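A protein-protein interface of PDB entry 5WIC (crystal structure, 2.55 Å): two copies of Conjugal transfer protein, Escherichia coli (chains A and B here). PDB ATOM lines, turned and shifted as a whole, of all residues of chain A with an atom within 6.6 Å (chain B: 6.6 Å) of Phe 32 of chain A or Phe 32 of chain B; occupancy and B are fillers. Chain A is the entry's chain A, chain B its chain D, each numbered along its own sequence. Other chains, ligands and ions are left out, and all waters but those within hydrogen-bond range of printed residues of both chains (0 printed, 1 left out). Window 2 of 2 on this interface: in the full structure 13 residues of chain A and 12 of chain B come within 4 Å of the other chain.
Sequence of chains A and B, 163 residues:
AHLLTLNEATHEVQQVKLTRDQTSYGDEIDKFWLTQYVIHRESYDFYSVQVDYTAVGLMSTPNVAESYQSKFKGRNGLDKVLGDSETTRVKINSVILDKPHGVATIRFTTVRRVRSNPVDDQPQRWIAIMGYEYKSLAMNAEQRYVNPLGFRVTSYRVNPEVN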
ATOM      1  N   ASP A  27       8.089 -23.466   4.919  1.00  0.00           N
ATOM      2  CA  ASP A  27       7.662 -23.883   6.248  1.00  0.00           C
ATOM      3  C   ASP A  27       6.984 -22.777   7.051  1.00  0.00           C
ATOM      4  O   ASP A  27       5.842 -22.927   7.479  1.00  0.00           O
ATOM      5  CB  ASP A  27       8.864 -24.409   7.037  1.00  0.00           C
ATOM      6  CG  ASP A  27       9.063 -25.906   6.884  1.00  0.00           C
ATOM      7  OD1 ASP A  27       8.458 -26.512   5.978  1.00  0.00           O
ATOM      8  OD2 ASP A  27       9.840 -26.483   7.671  1.00  0.00           O
ATOM      9  N   GLU A  28       7.682 -21.666   7.253  1.00  0.00           N
ATOM     10  CA  GLU A  28       7.218 -20.655   8.195  1.00  0.00           C
ATOM     11  C   GLU A  28       6.048 -19.830   7.665  1.00  0.00           C
ATOM     12  O   GLU A  28       5.226 -19.343   8.443  1.00  0.00           O
ATOM     13  CB  GLU A  28       8.375 -19.734   8.580  1.00  0.00           C
ATOM     14  CG  GLU A  28       9.497 -20.455   9.315  1.00  0.00           C
ATOM     15  CD  GLU A  28       9.003 -21.212  10.541  1.00  0.00           C
ATOM     16  OE1 GLU A  28       8.189 -20.650  11.306  1.00  0.00           O
ATOM     17  OE2 GLU A  28       9.420 -22.375  10.732  1.00  0.00           O
ATOM     18  N   ILE A  29       5.967 -19.678   6.348  1.00  0.00           N
ATOM     19  CA  ILE A  29       4.880 -18.911   5.752  1.00  0.00           C
ATOM     20  C   ILE A  29       3.617 -19.762   5.714  1.00  0.00           C
ATOM     21  O   ILE A  29       2.533 -19.285   6.043  1.00  0.00           O
ATOM     22  CB  ILE A  29       5.237 -18.417   4.335  1.00  0.00           C
ATOM     23  CG1 ILE A  29       6.505 -17.558   4.396  1.00  0.00           C
ATOM     24  CG2 ILE A  29       4.071 -17.627   3.735  1.00  0.00           C
ATOM     25  CD1 ILE A  29       6.949 -16.971   3.070  1.00  0.00           C
ATOM     26  N   ASP A  30       3.766 -21.022   5.317  1.00  0.00           N
ATOM     27  CA  ASP A  30       2.650 -21.961   5.309  1.00  0.00           C
ATOM     28  C   ASP A  30       2.041 -22.080   6.698  1.00  0.00           C
ATOM     29  O   ASP A  30       0.826 -21.995   6.865  1.00  0.00           O
ATOM     30  CB  ASP A  30       3.103 -23.340   4.829  1.00  0.00           C
ATOM     31  CG  ASP A  30       3.404 -23.371   3.355  1.00  0.00           C
ATOM     32  OD1 ASP A  30       3.403 -22.292   2.728  1.00  0.00           O
ATOM     33  OD2 ASP A  30       3.648 -24.476   2.825  1.00  0.00           O
ATOM     34  N   LYS A  31       2.908 -22.269   7.688  1.00  0.00           N
ATOM     35  CA  LYS A  31       2.495 -22.447   9.069  1.00  0.00           C
ATOM     36  C   LYS A  31       1.714 -21.238   9.577  1.00  0.00           C
ATOM     37  O   LYS A  31       0.772 -21.383  10.349  1.00  0.00           O
ATOM     38  CB  LYS A  31       3.724 -22.707   9.950  1.00  0.00           C
ATOM     39  CG  LYS A  31       3.440 -22.753  11.442  1.00  0.00           C
ATOM     40  CD  LYS A  31       4.696 -23.059  12.239  1.00  0.00           C
ATOM     41  CE  LYS A  31       4.462 -22.877  13.733  1.00  0.00           C
ATOM     42  NZ  LYS A  31       5.714 -23.042  14.524  1.00  0.00           N
ATOM     43  N   PHE A  32       2.097 -20.045   9.136  1.00  0.00           N
ATOM     44  CA  PHE A  32       1.421 -18.833   9.584  1.00  0.00           C
ATOM     45  C   PHE A  32      -0.044 -18.817   9.169  1.00  0.00           C
ATOM     46  O   PHE A  32      -0.922 -18.597   9.996  1.00  0.00           O
ATOM     47  CB  PHE A  32       2.113 -17.585   9.037  1.00  0.00           C
ATOM     48  CG  PHE A  32       1.340 -16.317   9.277  1.00  0.00           C
ATOM     49  CD1 PHE A  32       1.302 -15.743  10.532  1.00  0.00           C
ATOM     50  CD2 PHE A  32       0.647 -15.704   8.249  1.00  0.00           C
ATOM     51  CE1 PHE A  32       0.587 -14.582  10.755  1.00  0.00           C
ATOM     52  CE2 PHE A  32      -0.065 -14.545   8.469  1.00  0.00           C
ATOM     53  CZ  PHE A  32      -0.095 -13.984   9.722  1.00  0.00           C
ATOM     54  N   TRP A  33      -0.305 -19.045   7.899  1.00  0.00           N
ATOM     55  CA  TRP A  33      -1.632 -19.056   7.377  1.00  0.00           C
ATOM     56  C   TRP A  33      -2.455 -20.164   7.909  1.00  0.00           C
ATOM     57  O   TRP A  33      -3.600 -19.980   8.257  1.00  0.00           O
ATOM     58  CB  TRP A  33      -1.614 -19.076   5.855  1.00  0.00           C
ATOM     59  CG  TRP A  33      -0.974 -17.864   5.255  1.00  0.00           C
ATOM     60  CD1 TRP A  33       0.196 -17.797   4.551  1.00  0.00           C
ATOM     61  CD2 TRP A  33      -1.444 -16.500   5.306  1.00  0.00           C
ATOM     62  NE1 TRP A  33       0.471 -16.535   4.193  1.00  0.00           N
ATOM     63  CE2 TRP A  33      -0.468 -15.712   4.614  1.00  0.00           C
ATOM     64  CE3 TRP A  33      -2.520 -15.880   5.846  1.00  0.00           C
ATOM     65  CZ2 TRP A  33      -0.599 -14.368   4.473  1.00  0.00           C
ATOM     66  CZ3 TRP A  33      -2.638 -14.527   5.705  1.00  0.00           C
ATOM     67  CH2 TRP A  33      -1.704 -13.792   5.030  1.00  0.00           C
ATOM     68  N   LEU A  34      -1.869 -21.331   7.998  1.00  0.00           N
ATOM     69  CA  LEU A  34      -2.557 -22.520   8.476  1.00  0.00           C
ATOM     70  C   LEU A  34      -3.021 -22.352   9.920  1.00  0.00           C
ATOM     71  O   LEU A  34      -4.169 -22.643  10.241  1.00  0.00           O
ATOM     72  CB  LEU A  34      -1.655 -23.745   8.360  1.00  0.00           C
ATOM     73  CG  LEU A  34      -1.383 -24.274   6.952  1.00  0.00           C
ATOM     74  CD1 LEU A  34      -0.221 -25.251   6.975  1.00  0.00           C
ATOM     75  CD2 LEU A  34      -2.621 -24.947   6.397  1.00  0.00           C
ATOM     76  N   THR A  35      -2.129 -21.882  10.786  1.00  0.00           N
ATOM     77  CA  THR A  35      -2.483 -21.653  12.178  1.00  0.00           C
ATOM     78  C   THR A  35      -3.450 -20.475  12.303  1.00  0.00           C
ATOM     79  O   THR A  35      -4.306 -20.462  13.183  1.00  0.00           O
ATOM     80  CB  THR A  35      -1.230 -21.392  13.053  1.00  0.00           C
ATOM     81  OG1 THR A  35      -0.520 -20.246  12.572  1.00  0.00           O
ATOM     82  CG2 THR A  35      -0.308 -22.600  13.047  1.00  0.00           C
ATOM     83  N   GLN A  36      -3.313 -19.494  11.418  1.00  0.00           N
ATOM     84  CA  GLN A  36      -4.227 -18.353  11.393  1.00  0.00           C
ATOM     85  C   GLN A  36      -5.632 -18.793  10.997  1.00  0.00           C
ATOM     86  O   GLN A  36      -6.625 -18.277  11.504  1.00  0.00           O
ATOM     87  CB  GLN A  36      -3.728 -17.283  10.420  1.00  0.00           C
ATOM     88  CG  GLN A  36      -2.713 -16.333  11.022  1.00  0.00           C
ATOM     89  CD  GLN A  36      -3.336 -15.392  12.026  1.00  0.00           C
ATOM     90  OE1 GLN A  36      -2.950 -15.368  13.192  1.00  0.00           O
ATOM     91  NE2 GLN A  36      -4.305 -14.607  11.575  1.00  0.00           N
ATOM     92  N   TYR A  37      -5.701 -19.744  10.076  1.00  0.00           N
ATOM     93  CA  TYR A  37      -6.970 -20.283   9.627  1.00  0.00           C
ATOM     94  C   TYR A  37      -7.682 -20.996  10.771  1.00  0.00           C
ATOM     95  O   TYR A  37      -8.861 -20.757  11.027  1.00  0.00           O
ATOM     96  CB  TYR A  37      -6.753 -21.240   8.458  1.00  0.00           C
ATOM     97  CG  TYR A  37      -8.031 -21.761   7.849  1.00  0.00           C
ATOM     98  CD1 TYR A  37      -8.665 -21.070   6.827  1.00  0.00           C
ATOM     99  CD2 TYR A  37      -8.605 -22.943   8.296  1.00  0.00           C
ATOM    100  CE1 TYR A  37      -9.835 -21.541   6.267  1.00  0.00           C
ATOM    101  CE2 TYR A  37      -9.775 -23.423   7.740  1.00  0.00           C
ATOM    102  CZ  TYR A  37     -10.386 -22.716   6.725  1.00  0.00           C
ATOM    103  OH  TYR A  37     -11.551 -23.184   6.166  1.00  0.00           O
ATOM    104  N   ASP B  27      -2.788  -6.527  11.227  1.00  0.00           N
ATOM    105  CA  ASP B  27      -1.915  -6.646  12.384  1.00  0.00           C
ATOM    106  C   ASP B  27      -1.202  -7.993  12.460  1.00  0.00           C
ATOM    107  O   ASP B  27       0.015  -8.043  12.640  1.00  0.00           O
ATOM    108  CB  ASP B  27      -2.718  -6.410  13.661  1.00  0.00           C
ATOM    109  CG  ASP B  27      -3.103  -4.959  13.840  1.00  0.00           C
ATOM    110  OD1 ASP B  27      -3.177  -4.238  12.824  1.00  0.00           O
ATOM    111  OD2 ASP B  27      -3.326  -4.538  14.995  1.00  0.00           O
ATOM    112  N   GLU B  28      -1.950  -9.082  12.321  1.00  0.00           N
ATOM    113  CA  GLU B  28      -1.371 -10.412  12.479  1.00  0.00           C
ATOM    114  C   GLU B  28      -0.330 -10.687  11.406  1.00  0.00           C
ATOM    115  O   GLU B  28       0.670 -11.358  11.659  1.00  0.00           O
ATOM    116  CB  GLU B  28      -2.464 -11.481  12.444  1.00  0.00           C
ATOM    117  CG  GLU B  28      -3.445 -11.375  13.599  1.00  0.00           C
ATOM    118  CD  GLU B  28      -2.749 -11.321  14.941  1.00  0.00           C
ATOM    119  OE1 GLU B  28      -1.914 -12.211  15.216  1.00  0.00           O
ATOM    120  OE2 GLU B  28      -3.021 -10.380  15.716  1.00  0.00           O
ATOM    121  N   ILE B  29      -0.566 -10.161  10.210  1.00  0.00           N
ATOM    122  CA  ILE B  29       0.396 -10.293   9.129  1.00  0.00           C
ATOM    123  C   ILE B  29       1.625  -9.435   9.421  1.00  0.00           C
ATOM    124  O   ILE B  29       2.753  -9.849   9.159  1.00  0.00           O
ATOM    125  CB  ILE B  29      -0.226  -9.900   7.777  1.00  0.00           C
ATOM    126  CG1 ILE B  29      -1.422 -10.815   7.486  1.00  0.00           C
ATOM    127  CG2 ILE B  29       0.821  -9.980   6.664  1.00  0.00           C
ATOM    128  CD1 ILE B  29      -2.061 -10.636   6.120  1.00  0.00           C
ATOM    129  N   ASP B  30       1.405  -8.246   9.972  1.00  0.00           N
ATOM    130  CA  ASP B  30       2.507  -7.374  10.367  1.00  0.00           C
ATOM    131  C   ASP B  30       3.360  -8.035  11.443  1.00  0.00           C
ATOM    132  O   ASP B  30       4.588  -8.009  11.376  1.00  0.00           O
ATOM    133  CB  ASP B  30       1.982  -6.027  10.877  1.00  0.00           C
ATOM    134  CG  ASP B  30       1.680  -5.045   9.757  1.00  0.00           C
ATOM    135  OD1 ASP B  30       1.803  -5.416   8.569  1.00  0.00           O
ATOM    136  OD2 ASP B  30       1.311  -3.894  10.070  1.00  0.00           O
ATOM    137  N   LYS B  31       2.704  -8.633  12.432  1.00  0.00           N
ATOM    138  CA  LYS B  31       3.407  -9.242  13.553  1.00  0.00           C
ATOM    139  C   LYS B  31       4.272 -10.421  13.114  1.00  0.00           C
ATOM    140  O   LYS B  31       5.324 -10.680  13.699  1.00  0.00           O
ATOM    141  CB  LYS B  31       2.410  -9.696  14.619  1.00  0.00           C
ATOM    142  CG  LYS B  31       1.757  -8.553  15.377  1.00  0.00           C
ATOM    143  CD  LYS B  31       0.758  -9.068  16.391  1.00  0.00           C
ATOM    144  CE  LYS B  31       0.114  -7.936  17.168  1.00  0.00           C
ATOM    145  NZ  LYS B  31      -0.804  -8.450  18.222  1.00  0.00           N
ATOM    146  N   PHE B  32       3.828 -11.137  12.087  1.00  0.00           N
ATOM    147  CA  PHE B  32       4.574 -12.286  11.597  1.00  0.00           C
ATOM    148  C   PHE B  32       5.942 -11.878  11.067  1.00  0.00           C
ATOM    149  O   PHE B  32       6.968 -12.366  11.543  1.00  0.00           O
ATOM    150  CB  PHE B  32       3.795 -13.010  10.501  1.00  0.00           C
ATOM    151  CG  PHE B  32       4.534 -14.172   9.902  1.00  0.00           C
ATOM    152  CD1 PHE B  32       4.762 -15.319  10.642  1.00  0.00           C
ATOM    153  CD2 PHE B  32       5.000 -14.119   8.599  1.00  0.00           C
ATOM    154  CE1 PHE B  32       5.440 -16.389  10.098  1.00  0.00           C
ATOM    155  CE2 PHE B  32       5.678 -15.188   8.047  1.00  0.00           C
ATOM    156  CZ  PHE B  32       5.898 -16.324   8.797  1.00  0.00           C
ATOM    157  N   TRP B  33       5.951 -10.968  10.117  1.00  0.00           N
ATOM    158  CA  TRP B  33       7.170 -10.545   9.493  1.00  0.00           C
ATOM    159  C   TRP B  33       8.101  -9.899  10.440  1.00  0.00           C
ATOM    160  O   TRP B  33       9.290 -10.141  10.399  1.00  0.00           O
ATOM    161  CB  TRP B  33       6.868  -9.614   8.358  1.00  0.00           C
ATOM    162  CG  TRP B  33       6.101 -10.285   7.280  1.00  0.00           C
ATOM    163  CD1 TRP B  33       4.816 -10.033   6.881  1.00  0.00           C
ATOM    164  CD2 TRP B  33       6.545 -11.355   6.434  1.00  0.00           C
ATOM    165  NE1 TRP B  33       4.451 -10.854   5.873  1.00  0.00           N
ATOM    166  CE2 TRP B  33       5.437 -11.666   5.558  1.00  0.00           C
ATOM    167  CE3 TRP B  33       7.702 -12.058   6.311  1.00  0.00           C
ATOM    168  CZ2 TRP B  33       5.509 -12.644   4.622  1.00  0.00           C
ATOM    169  CZ3 TRP B  33       7.764 -13.043   5.358  1.00  0.00           C
ATOM    170  CH2 TRP B  33       6.689 -13.329   4.534  1.00  0.00           C
ATOM    171  N   LEU B  34       7.571  -9.077  11.313  1.00  0.00           N
ATOM    172  CA  LEU B  34       8.370  -8.389  12.318  1.00  0.00           C
ATOM    173  C   LEU B  34       9.077  -9.389  13.229  1.00  0.00           C
ATOM    174  O   LEU B  34      10.282  -9.282  13.452  1.00  0.00           O
ATOM    175  CB  LEU B  34       7.497  -7.445  13.146  1.00  0.00           C
ATOM    176  CG  LEU B  34       6.936  -6.227  12.408  1.00  0.00           C
ATOM    177  CD1 LEU B  34       5.792  -5.597  13.188  1.00  0.00           C
ATOM    178  CD2 LEU B  34       8.033  -5.208  12.169  1.00  0.00           C
ATOM    179  N   THR B  35       8.335 -10.366  13.743  1.00  0.00           N
ATOM    180  CA  THR B  35       8.916 -11.360  14.638  1.00  0.00           C
ATOM    181  C   THR B  35       9.889 -12.267  13.896  1.00  0.00           C
ATOM    182  O   THR B  35      10.933 -12.627  14.432  1.00  0.00           O
ATOM    183  CB  THR B  35       7.836 -12.229  15.315  1.00  0.00           C
ATOM    184  OG1 THR B  35       6.955 -12.777  14.327  1.00  0.00           O
ATOM    185  CG2 THR B  35       7.038 -11.402  16.298  1.00  0.00           C
ATOM    186  N   GLN B  36       9.544 -12.637  12.666  1.00  0.00           N
ATOM    187  CA  GLN B  36      10.429 -13.449  11.838  1.00  0.00           C
ATOM    188  C   GLN B  36      11.728 -12.707  11.544  1.00  0.00           C
ATOM    189  O   GLN B  36      12.788 -13.320  11.408  1.00  0.00           O
ATOM    190  CB  GLN B  36       9.739 -13.833  10.529  1.00  0.00           C
ATOM    191  CG  GLN B  36       8.663 -14.890  10.683  1.00  0.00           C
ATOM    192  CD  GLN B  36       9.232 -16.267  10.948  1.00  0.00           C
ATOM    193  OE1 GLN B  36      10.026 -16.785  10.163  1.00  0.00           O
ATOM    194  NE2 GLN B  36       8.830 -16.868  12.061  1.00  0.00           N
ATOM    195  N   TYR B  37      11.640 -11.384  11.447  1.00  0.00           N
ATOM    196  CA  TYR B  37      12.817 -10.554  11.220  1.00  0.00           C
ATOM    197  C   TYR B  37      13.747 -10.621  12.422  1.00  0.00           C
ATOM    198  O   TYR B  37      14.950 -10.835  12.273  1.00  0.00           O
ATOM    199  CB  TYR B  37      12.414  -9.106  10.947  1.00  0.00           C
ATOM    200  CG  TYR B  37      13.581  -8.186  10.671  1.00  0.00           C
ATOM    201  CD1 TYR B  37      14.132  -8.092   9.402  1.00  0.00           C
ATOM    202  CD2 TYR B  37      14.128  -7.407  11.681  1.00  0.00           C
ATOM    203  CE1 TYR B  37      15.197  -7.253   9.147  1.00  0.00           C
ATOM    204  CE2 TYR B  37      15.192  -6.564  11.435  1.00  0.00           C
ATOM    205  CZ  TYR B  37      15.723  -6.492  10.165  1.00  0.00           C
ATOM    206  OH  TYR B  37      16.782  -5.654   9.913  1.00  0.00           O
ATOM    207  N   MET B  59      14.632  -7.868   3.805  1.00  0.00           N
ATOM    208  CA  MET B  59      13.663  -7.288   4.727  1.00  0.00           C
ATOM    209  C   MET B  59      14.204  -6.036   5.413  1.00  0.00           C
ATOM    210  O   MET B  59      13.724  -5.649   6.478  1.00  0.00           O
ATOM    211  CB  MET B  59      13.249  -8.327   5.775  1.00  0.00           C
ATOM    212  CG  MET B  59      12.527  -9.535   5.193  1.00  0.00           C
ATOM    213  SD  MET B  59      12.309 -10.890   6.369  1.00  0.00           S
ATOM    214  CE  MET B  59      11.263 -10.133   7.603  1.00  0.00           C
ATOM    215  N   VAL B  95       4.513  -8.428  21.200  1.00  0.00           N
ATOM    216  CA  VAL B  95       4.599  -7.606  19.999  1.00  0.00           C
ATOM    217  C   VAL B  95       3.478  -6.570  19.987  1.00  0.00           C
ATOM    218  O   VAL B  95       2.319  -6.905  19.736  1.00  0.00           O
ATOM    219  CB  VAL B  95       4.506  -8.460  18.714  1.00  0.00           C
ATOM    220  CG1 VAL B  95       4.684  -7.592  17.476  1.00  0.00           C
ATOM    221  CG2 VAL B  95       5.537  -9.573  18.727  1.00  0.00           C
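Glu 28 of chain A touches Phe 32 of chain B, and with the chains exchanged Phe 32 of chain A touches Glu 28 of chain B.
Glu 28 of chain A touches Gln 36 of chain B, and with the chains exchanged Gln 36 of chain A touches Glu 28 of chain B.
Phe 32 of chain A touches Ile 29 of chain B, but with the chains exchanged Ile 29 of chain A does not touch Phe 32 of chain B (4.1 Å).
Phe 32 of chain A touches its own counterpart, Phe 32 of chain B.
11 positions are printed for both chains.
The side-chain amino group (NZ) of Lys 31 of chain B is in salt-bridge range of the side-chain carboxylate (OE2) of Glu 28 of chain B, 3.9 Å away.
The backbone carbonyl oxygen of Phe 32 of chain A lies within hydrogen-bond range of the side-chain hydroxyl of Thr 35 of chain A (3.1 Å).
The backbone carbonyl oxygen (O) of Phe 32 of chain B sits at hydrogen-bond distance from the side-chain hydroxyl (OG1) of Thr 35 of chain B, 2.8 Å away.
Of the 13 printed residues of chain B, 5 touch a printed residue of chain A.
Hydrophobic or aromatic side chains of chain B within 4 Å of the printed part of chain A: Ile 29, Phe 32 and Trp 33.
Along chain B the printed residues that touch a printed residue of chain A span positions 28 to 36.
Hydrophobic or aromatic side chains of chain A that line the printed part of chain B: Ile 29, Phe 32 and Trp 33.
Among the printed residues, 8 pairs touch across the chains.
Among the printed residues, no Asp or Glu carboxylate lies within 4 Å of a Lys or Arg side-chain nitrogen of the other chain.
Printed residues of chain B within 4 Å of Glu 28 of chain A: Phe 32 and Gln 36.
Of the printed residues of chain B, Ile 29 of chain A touches Trp 33.
Of chain B, only Glu 28, Ile 29 and Phe 32 come within 4 Å of Phe 32 of chain A.
Of the printed residues of chain B, Trp 33 of chain A touches Ile 29 (3.4 Å).
Asp 27 of chain B touches none of the printed residues of chain A.
Phe 32 of chain B touches two residues of chain A.
Printed residues of chain A within 4 Å of Trp 33 of chain B: Ile 29.
The nearest residue of chain B that does not touch Phe 32 of chain A is Asp 30 of chain B (5.9 Å).
The nearest residue of chain A that does not touch Phe 32 of chain B is Ile 29 of chain A (4.1 Å).
O of Glu 28 of chain A touches CZ of Phe 32 of chain B, at 3.1 Å.
Glu 28 of chain A touches Gln 36 of chain B.
CD1 of Ile 29 of chain A touches CH2 of Trp 33 of chain B, 3.9 Å away.
Glu 28 of chain B touches Phe 32 of chain A.
Phe 32 of chain A touches Ile 29 of chain B (CZ to CA, 3.8 Å).
Phe 32 of chain A touches Phe 32 of chain B (CD1 to CD1, 3.5 Å).
Trp 33 of chain A touches Ile 29 of chain B.
Gln 36 of chain A touches Glu 28 of chain B.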
